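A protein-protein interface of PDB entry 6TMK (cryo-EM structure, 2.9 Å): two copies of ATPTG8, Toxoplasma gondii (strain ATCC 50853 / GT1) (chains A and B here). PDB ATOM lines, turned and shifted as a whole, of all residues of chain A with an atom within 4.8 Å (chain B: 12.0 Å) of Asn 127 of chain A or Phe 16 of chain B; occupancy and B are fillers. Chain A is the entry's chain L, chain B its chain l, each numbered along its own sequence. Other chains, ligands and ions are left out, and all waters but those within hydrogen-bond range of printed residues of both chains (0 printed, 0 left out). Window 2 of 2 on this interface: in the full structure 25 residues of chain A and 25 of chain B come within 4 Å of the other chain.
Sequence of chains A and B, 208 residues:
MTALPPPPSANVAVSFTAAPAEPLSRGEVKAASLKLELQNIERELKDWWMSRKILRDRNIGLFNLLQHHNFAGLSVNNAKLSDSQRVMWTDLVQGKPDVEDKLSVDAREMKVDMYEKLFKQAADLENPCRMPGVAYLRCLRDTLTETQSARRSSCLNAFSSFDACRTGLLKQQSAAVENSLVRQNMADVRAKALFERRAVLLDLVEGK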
ATOM      1  N   ALA A 123      16.635 -15.395   0.374  1.00  0.00           N
ATOM      2  CA  ALA A 123      15.362 -15.951  -0.049  1.00  0.00           C
ATOM      3  C   ALA A 123      14.259 -15.463   0.873  1.00  0.00           C
ATOM      4  O   ALA A 123      14.352 -15.611   2.095  1.00  0.00           O
ATOM      5  CB  ALA A 123      15.416 -17.476  -0.041  1.00  0.00           C
ATOM      6  N   ASP A 124      13.222 -14.884   0.286  1.00  0.00           N
ATOM      7  CA  ASP A 124      12.068 -14.422   1.034  1.00  0.00           C
ATOM      8  C   ASP A 124      11.024 -15.528   1.138  1.00  0.00           C
ATOM      9  O   ASP A 124      11.165 -16.616   0.576  1.00  0.00           O
ATOM     10  CB  ASP A 124      11.478 -13.170   0.395  1.00  0.00           C
ATOM     11  CG  ASP A 124      11.021 -13.399  -1.028  1.00  0.00           C
ATOM     12  OD1 ASP A 124      11.420 -14.417  -1.625  1.00  0.00           O
ATOM     13  OD2 ASP A 124      10.257 -12.560  -1.549  1.00  0.00           O
ATOM     14  N   LEU A 125       9.960 -15.245   1.884  1.00  0.00           N
ATOM     15  CA  LEU A 125       8.953 -16.257   2.163  1.00  0.00           C
ATOM     16  C   LEU A 125       8.211 -16.679   0.903  1.00  0.00           C
ATOM     17  O   LEU A 125       7.690 -17.799   0.838  1.00  0.00           O
ATOM     18  CB  LEU A 125       7.973 -15.732   3.203  1.00  0.00           C
ATOM     19  CG  LEU A 125       8.567 -15.520   4.593  1.00  0.00           C
ATOM     20  CD1 LEU A 125       7.770 -14.509   5.381  1.00  0.00           C
ATOM     21  CD2 LEU A 125       8.623 -16.829   5.337  1.00  0.00           C
ATOM     22  N   GLU A 126       8.139 -15.800  -0.098  1.00  0.00           N
ATOM     23  CA  GLU A 126       7.552 -16.174  -1.375  1.00  0.00           C
ATOM     24  C   GLU A 126       8.435 -17.133  -2.161  1.00  0.00           C
ATOM     25  O   GLU A 126       7.944 -17.792  -3.082  1.00  0.00           O
ATOM     26  CB  GLU A 126       7.300 -14.918  -2.204  1.00  0.00           C
ATOM     27  CG  GLU A 126       6.513 -13.849  -1.468  1.00  0.00           C
ATOM     28  CD  GLU A 126       6.076 -12.715  -2.371  1.00  0.00           C
ATOM     29  OE1 GLU A 126       6.858 -12.328  -3.263  1.00  0.00           O
ATOM     30  OE2 GLU A 126       4.951 -12.204  -2.181  1.00  0.00           O
ATOM     31  N   ASN A 127       9.716 -17.216  -1.826  1.00  0.00           N
ATOM     32  CA  ASN A 127      10.625 -18.078  -2.558  1.00  0.00           C
ATOM     33  C   ASN A 127      10.287 -19.544  -2.286  1.00  0.00           C
ATOM     34  O   ASN A 127       9.997 -19.910  -1.145  1.00  0.00           O
ATOM     35  CB  ASN A 127      12.064 -17.781  -2.157  1.00  0.00           C
ATOM     36  CG  ASN A 127      13.071 -18.342  -3.126  1.00  0.00           C
ATOM     37  OD1 ASN A 127      13.049 -19.524  -3.458  1.00  0.00           O
ATOM     38  ND2 ASN A 127      13.967 -17.491  -3.586  1.00  0.00           N
ATOM     39  N   PRO A 128      10.308 -20.405  -3.305  1.00  0.00           N
ATOM     40  CA  PRO A 128      10.009 -21.820  -3.046  1.00  0.00           C
ATOM     41  C   PRO A 128      11.122 -22.569  -2.330  1.00  0.00           C
ATOM     42  O   PRO A 128      10.825 -23.501  -1.574  1.00  0.00           O
ATOM     43  CB  PRO A 128       9.769 -22.390  -4.451  1.00  0.00           C
ATOM     44  CG  PRO A 128       9.546 -21.220  -5.318  1.00  0.00           C
ATOM     45  CD  PRO A 128      10.344 -20.121  -4.746  1.00  0.00           C
ATOM     46  N   CYS A 129      12.386 -22.213  -2.549  1.00  0.00           N
ATOM     47  CA  CYS A 129      13.488 -22.968  -1.968  1.00  0.00           C
ATOM     48  C   CYS A 129      13.739 -22.628  -0.504  1.00  0.00           C
ATOM     49  O   CYS A 129      14.568 -23.288   0.140  1.00  0.00           O
ATOM     50  CB  CYS A 129      14.764 -22.725  -2.776  1.00  0.00           C
ATOM     51  SG  CYS A 129      14.583 -22.892  -4.567  1.00  0.00           S
ATOM     52  N   ARG A 130      13.028 -21.641   0.040  1.00  0.00           N
ATOM     53  CA  ARG A 130      13.269 -21.211   1.411  1.00  0.00           C
ATOM     54  C   ARG A 130      12.983 -22.320   2.411  1.00  0.00           C
ATOM     55  O   ARG A 130      13.785 -22.572   3.317  1.00  0.00           O
ATOM     56  CB  ARG A 130      12.422 -19.986   1.724  1.00  0.00           C
ATOM     57  CG  ARG A 130      12.832 -19.283   2.989  1.00  0.00           C
ATOM     58  CD  ARG A 130      11.719 -18.448   3.519  1.00  0.00           C
ATOM     59  NE  ARG A 130      11.972 -17.987   4.876  1.00  0.00           N
ATOM     60  CZ  ARG A 130      12.733 -16.948   5.189  1.00  0.00           C
ATOM     61  NH1 ARG A 130      13.335 -16.250   4.247  1.00  0.00           N
ATOM     62  NH2 ARG A 130      12.896 -16.611   6.451  1.00  0.00           N
ATOM     63  N   LEU A 169      15.409 -23.461 -10.300  1.00  0.00           N
ATOM     64  CA  LEU A 169      15.671 -22.039 -10.499  1.00  0.00           C
ATOM     65  C   LEU A 169      16.719 -21.815 -11.582  1.00  0.00           C
ATOM     66  O   LEU A 169      16.582 -20.912 -12.421  1.00  0.00           O
ATOM     67  CB  LEU A 169      16.124 -21.407  -9.191  1.00  0.00           C
ATOM     68  CG  LEU A 169      15.149 -21.437  -8.021  1.00  0.00           C
ATOM     69  CD1 LEU A 169      15.642 -20.514  -6.949  1.00  0.00           C
ATOM     70  CD2 LEU A 169      13.759 -21.057  -8.432  1.00  0.00           C
ATOM     71  N   GLN A 172      15.182 -22.319 -14.904  1.00  0.00           N
ATOM     72  CA  GLN A 172      14.332 -21.176 -15.211  1.00  0.00           C
ATOM     73  C   GLN A 172      15.147 -20.025 -15.774  1.00  0.00           C
ATOM     74  O   GLN A 172      14.760 -19.397 -16.765  1.00  0.00           O
ATOM     75  CB  GLN A 172      13.605 -20.727 -13.951  1.00  0.00           C
ATOM     76  CG  GLN A 172      12.429 -21.567 -13.578  1.00  0.00           C
ATOM     77  CD  GLN A 172      11.769 -21.099 -12.312  1.00  0.00           C
ATOM     78  OE1 GLN A 172      12.371 -20.398 -11.506  1.00  0.00           O
ATOM     79  NE2 GLN A 172      10.522 -21.477 -12.130  1.00  0.00           N
ATOM     80  N   ALA B  10      -4.600 -14.580  -8.448  1.00  0.00           N
ATOM     81  CA  ALA B  10      -4.232 -15.536  -7.420  1.00  0.00           C
ATOM     82  C   ALA B  10      -4.242 -14.878  -6.050  1.00  0.00           C
ATOM     83  O   ALA B  10      -3.882 -13.708  -5.901  1.00  0.00           O
ATOM     84  CB  ALA B  10      -2.853 -16.116  -7.713  1.00  0.00           C
ATOM     85  N   VAL B  12      -2.672 -16.459  -3.260  1.00  0.00           N
ATOM     86  CA  VAL B  12      -1.291 -16.692  -2.875  1.00  0.00           C
ATOM     87  C   VAL B  12      -0.387 -16.103  -3.944  1.00  0.00           C
ATOM     88  O   VAL B  12      -0.700 -16.146  -5.139  1.00  0.00           O
ATOM     89  CB  VAL B  12      -1.028 -18.194  -2.683  1.00  0.00           C
ATOM     90  CG1 VAL B  12       0.440 -18.446  -2.452  1.00  0.00           C
ATOM     91  CG2 VAL B  12      -1.847 -18.732  -1.539  1.00  0.00           C
ATOM     92  N   ALA B  13       0.739 -15.548  -3.520  1.00  0.00           N
ATOM     93  CA  ALA B  13       1.627 -14.850  -4.435  1.00  0.00           C
ATOM     94  C   ALA B  13       2.465 -15.851  -5.215  1.00  0.00           C
ATOM     95  O   ALA B  13       3.212 -16.637  -4.624  1.00  0.00           O
ATOM     96  CB  ALA B  13       2.526 -13.889  -3.665  1.00  0.00           C
ATOM     97  N   VAL B  14       2.340 -15.824  -6.537  1.00  0.00           N
ATOM     98  CA  VAL B  14       3.252 -16.528  -7.422  1.00  0.00           C
ATOM     99  C   VAL B  14       4.296 -15.515  -7.864  1.00  0.00           C
ATOM    100  O   VAL B  14       3.958 -14.476  -8.444  1.00  0.00           O
ATOM    101  CB  VAL B  14       2.519 -17.145  -8.625  1.00  0.00           C
ATOM    102  CG1 VAL B  14       1.565 -18.224  -8.172  1.00  0.00           C
ATOM    103  CG2 VAL B  14       1.772 -16.085  -9.426  1.00  0.00           C
ATOM    104  N   SER B  15       5.558 -15.795  -7.560  1.00  0.00           N
ATOM    105  CA  SER B  15       6.640 -14.888  -7.922  1.00  0.00           C
ATOM    106  C   SER B  15       7.287 -15.288  -9.245  1.00  0.00           C
ATOM    107  O   SER B  15       7.199 -14.557 -10.235  1.00  0.00           O
ATOM    108  CB  SER B  15       7.661 -14.839  -6.780  1.00  0.00           C
ATOM    109  OG  SER B  15       8.289 -16.092  -6.584  1.00  0.00           O
ATOM    110  N   PHE B  16       7.920 -16.458  -9.274  1.00  0.00           N
ATOM    111  CA  PHE B  16       8.528 -16.979 -10.489  1.00  0.00           C
ATOM    112  C   PHE B  16       8.355 -18.486 -10.580  1.00  0.00           C
ATOM    113  O   PHE B  16       8.927 -19.109 -11.482  1.00  0.00           O
ATOM    114  CB  PHE B  16      10.014 -16.631 -10.546  1.00  0.00           C
ATOM    115  CG  PHE B  16      10.729 -16.833  -9.249  1.00  0.00           C
ATOM    116  CD1 PHE B  16      11.136 -18.092  -8.865  1.00  0.00           C
ATOM    117  CD2 PHE B  16      11.014 -15.768  -8.423  1.00  0.00           C
ATOM    118  CE1 PHE B  16      11.793 -18.287  -7.682  1.00  0.00           C
ATOM    119  CE2 PHE B  16      11.673 -15.964  -7.234  1.00  0.00           C
ATOM    120  CZ  PHE B  16      12.062 -17.224  -6.867  1.00  0.00           C
ATOM    121  N   THR B  17       7.581 -19.082  -9.675  1.00  0.00           N
ATOM    122  CA  THR B  17       7.487 -20.531  -9.593  1.00  0.00           C
ATOM    123  C   THR B  17       6.905 -21.131 -10.863  1.00  0.00           C
ATOM    124  O   THR B  17       7.239 -22.266 -11.222  1.00  0.00           O
ATOM    125  CB  THR B  17       6.630 -20.892  -8.384  1.00  0.00           C
ATOM    126  OG1 THR B  17       7.058 -20.118  -7.258  1.00  0.00           O
ATOM    127  CG2 THR B  17       6.764 -22.354  -8.049  1.00  0.00           C
ATOM    128  N   ALA B  18       6.044 -20.393 -11.554  1.00  0.00           N
ATOM    129  CA  ALA B  18       5.396 -20.867 -12.765  1.00  0.00           C
ATOM    130  C   ALA B  18       6.205 -20.598 -14.023  1.00  0.00           C
ATOM    131  O   ALA B  18       5.730 -20.904 -15.120  1.00  0.00           O
ATOM    132  CB  ALA B  18       4.022 -20.221 -12.904  1.00  0.00           C
ATOM    133  N   ALA B  19       7.401 -20.038 -13.899  1.00  0.00           N
ATOM    134  CA  ALA B  19       8.184 -19.726 -15.074  1.00  0.00           C
ATOM    135  C   ALA B  19       8.647 -21.006 -15.764  1.00  0.00           C
ATOM    136  O   ALA B  19       8.827 -22.041 -15.119  1.00  0.00           O
ATOM    137  CB  ALA B  19       9.390 -18.881 -14.695  1.00  0.00           C
ATOM    138  N   PRO B  20       8.846 -20.962 -17.078  1.00  0.00           N
ATOM    139  CA  PRO B  20       9.262 -22.170 -17.794  1.00  0.00           C
ATOM    140  C   PRO B  20      10.682 -22.578 -17.447  1.00  0.00           C
ATOM    141  O   PRO B  20      11.571 -21.739 -17.290  1.00  0.00           O
ATOM    142  CB  PRO B  20       9.136 -21.767 -19.266  1.00  0.00           C
ATOM    143  CG  PRO B  20       9.221 -20.299 -19.266  1.00  0.00           C
ATOM    144  CD  PRO B  20       8.592 -19.845 -17.999  1.00  0.00           C
ATOM    145  N   ALA B  21      10.884 -23.885 -17.321  1.00  0.00           N
ATOM    146  CA  ALA B  21      12.195 -24.458 -17.075  1.00  0.00           C
ATOM    147  C   ALA B  21      12.811 -25.040 -18.335  1.00  0.00           C
ATOM    148  O   ALA B  21      13.810 -25.759 -18.251  1.00  0.00           O
ATOM    149  CB  ALA B  21      12.100 -25.534 -16.000  1.00  0.00           C
ATOM    150  N   GLU B  22      12.238 -24.744 -19.500  1.00  0.00           N
ATOM    151  CA  GLU B  22      12.695 -25.281 -20.757  1.00  0.00           C
ATOM    152  C   GLU B  22      12.463 -24.218 -21.818  1.00  0.00           C
ATOM    153  O   GLU B  22      11.434 -23.530 -21.775  1.00  0.00           O
ATOM    154  CB  GLU B  22      11.951 -26.567 -21.125  1.00  0.00           C
ATOM    155  CG  GLU B  22      12.625 -27.397 -22.198  1.00  0.00           C
ATOM    156  CD  GLU B  22      11.956 -28.741 -22.401  1.00  0.00           C
ATOM    157  OE1 GLU B  22      12.607 -29.651 -22.956  1.00  0.00           O
ATOM    158  OE2 GLU B  22      10.780 -28.891 -22.005  1.00  0.00           O
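NE2 of Gln 172 of chain A lies within hydrogen-bond range of O of Phe 16 of chain B.
The backbone carbonyl oxygen (O) of Thr 17 of chain B lies within hydrogen-bond range of the side-chain amide nitrogen (NE2) of Gln 172 of chain A.
The backbone carbonyl oxygen (O) of Ala 19 of chain B is in hydrogen-bond range of the side-chain amide nitrogen (NE2) of Gln 172 of chain A (3.5 Å).
N of Asn 127 of chain A sits at hydrogen-bond distance from OD1 of Asp 124 of chain A, 3.3 Å away.
The backbone NH (N) of Cys 129 of chain A lies within hydrogen-bond range of the side-chain amide oxygen (OD1) of Asn 127 of chain A (2.9 Å).
Among the printed residues, pairs that only touch across the chains: Glu 126 of chain A with Ala 13 of chain B (3.3 Å), Glu 126 of chain A with Ser 15 of chain B (3.9 Å), Asn 127 of chain A with Phe 16 of chain B (3.8 Å), Pro 128 of chain A with Phe 16 of chain B (3.8 Å), Pro 128 of chain A with Thr 17 of chain B (3.3 Å), Leu 169 of chain A with Phe 16 of chain B (3.5 Å) and Gln 172 of chain A with Pro 20 of chain B (3.5 Å).
No residue of chain B comes within 4 Å of Leu 125 of chain A.
Asn 127 of chain A touches just one residue of chain B: Phe 16 (3.8 Å).
Of chain B, only Phe 16 and Thr 17 come within 4 Å of Pro 128 of chain A.
Leu 169 of chain A touches one residue of chain B.
Printed residues of chain A within 4 Å of Ala 13 of chain B: Glu 126 (3.3 Å).
Val 14 of chain B touches none of the printed residues of chain A.
Of the printed residues of chain A, Ser 15 of chain B touches Glu 126.
Of chain A, only Asn 127 (3.8 Å), Pro 128 (3.8 Å), Leu 169 (3.5 Å) and Gln 172 (2.9 Å) come within 4 Å of Phe 16 of chain B.
Of the printed residues of chain A, Thr 17 of chain B touches Pro 128 (3.3 Å) and Gln 172 (3.5 Å).
Printed residues of chain A within 4 Å of Pro 20 of chain B: Gln 172.
The nearest printed residue of chain A that does not touch Phe 16 of chain B is Glu 126 of chain A (5.6 Å).
Of the 12 printed residues of chain B, 6 touch a printed residue of chain A.
Hydrophobic or aromatic side chains of chain B that line the printed part of chain A: Ala 13, Phe 16 and Ala 19.
Of the 10 printed residues of chain A, 5 touch a printed residue of chain B.
Hydrophobic or aromatic side chains of chain A that line the printed part of chain B: Pro 128 and Leu 169.
Among the printed residues, 10 pairs touch across the chains.
Among the printed residues, no Asp or Glu carboxylate lies within 4 Å of a Lys or Arg side-chain nitrogen of the other chain.
No position is printed for both chains.
Of the 10 pairs that touch across the chains among the printed residues, none has its exchanged pair printed and touching as well.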
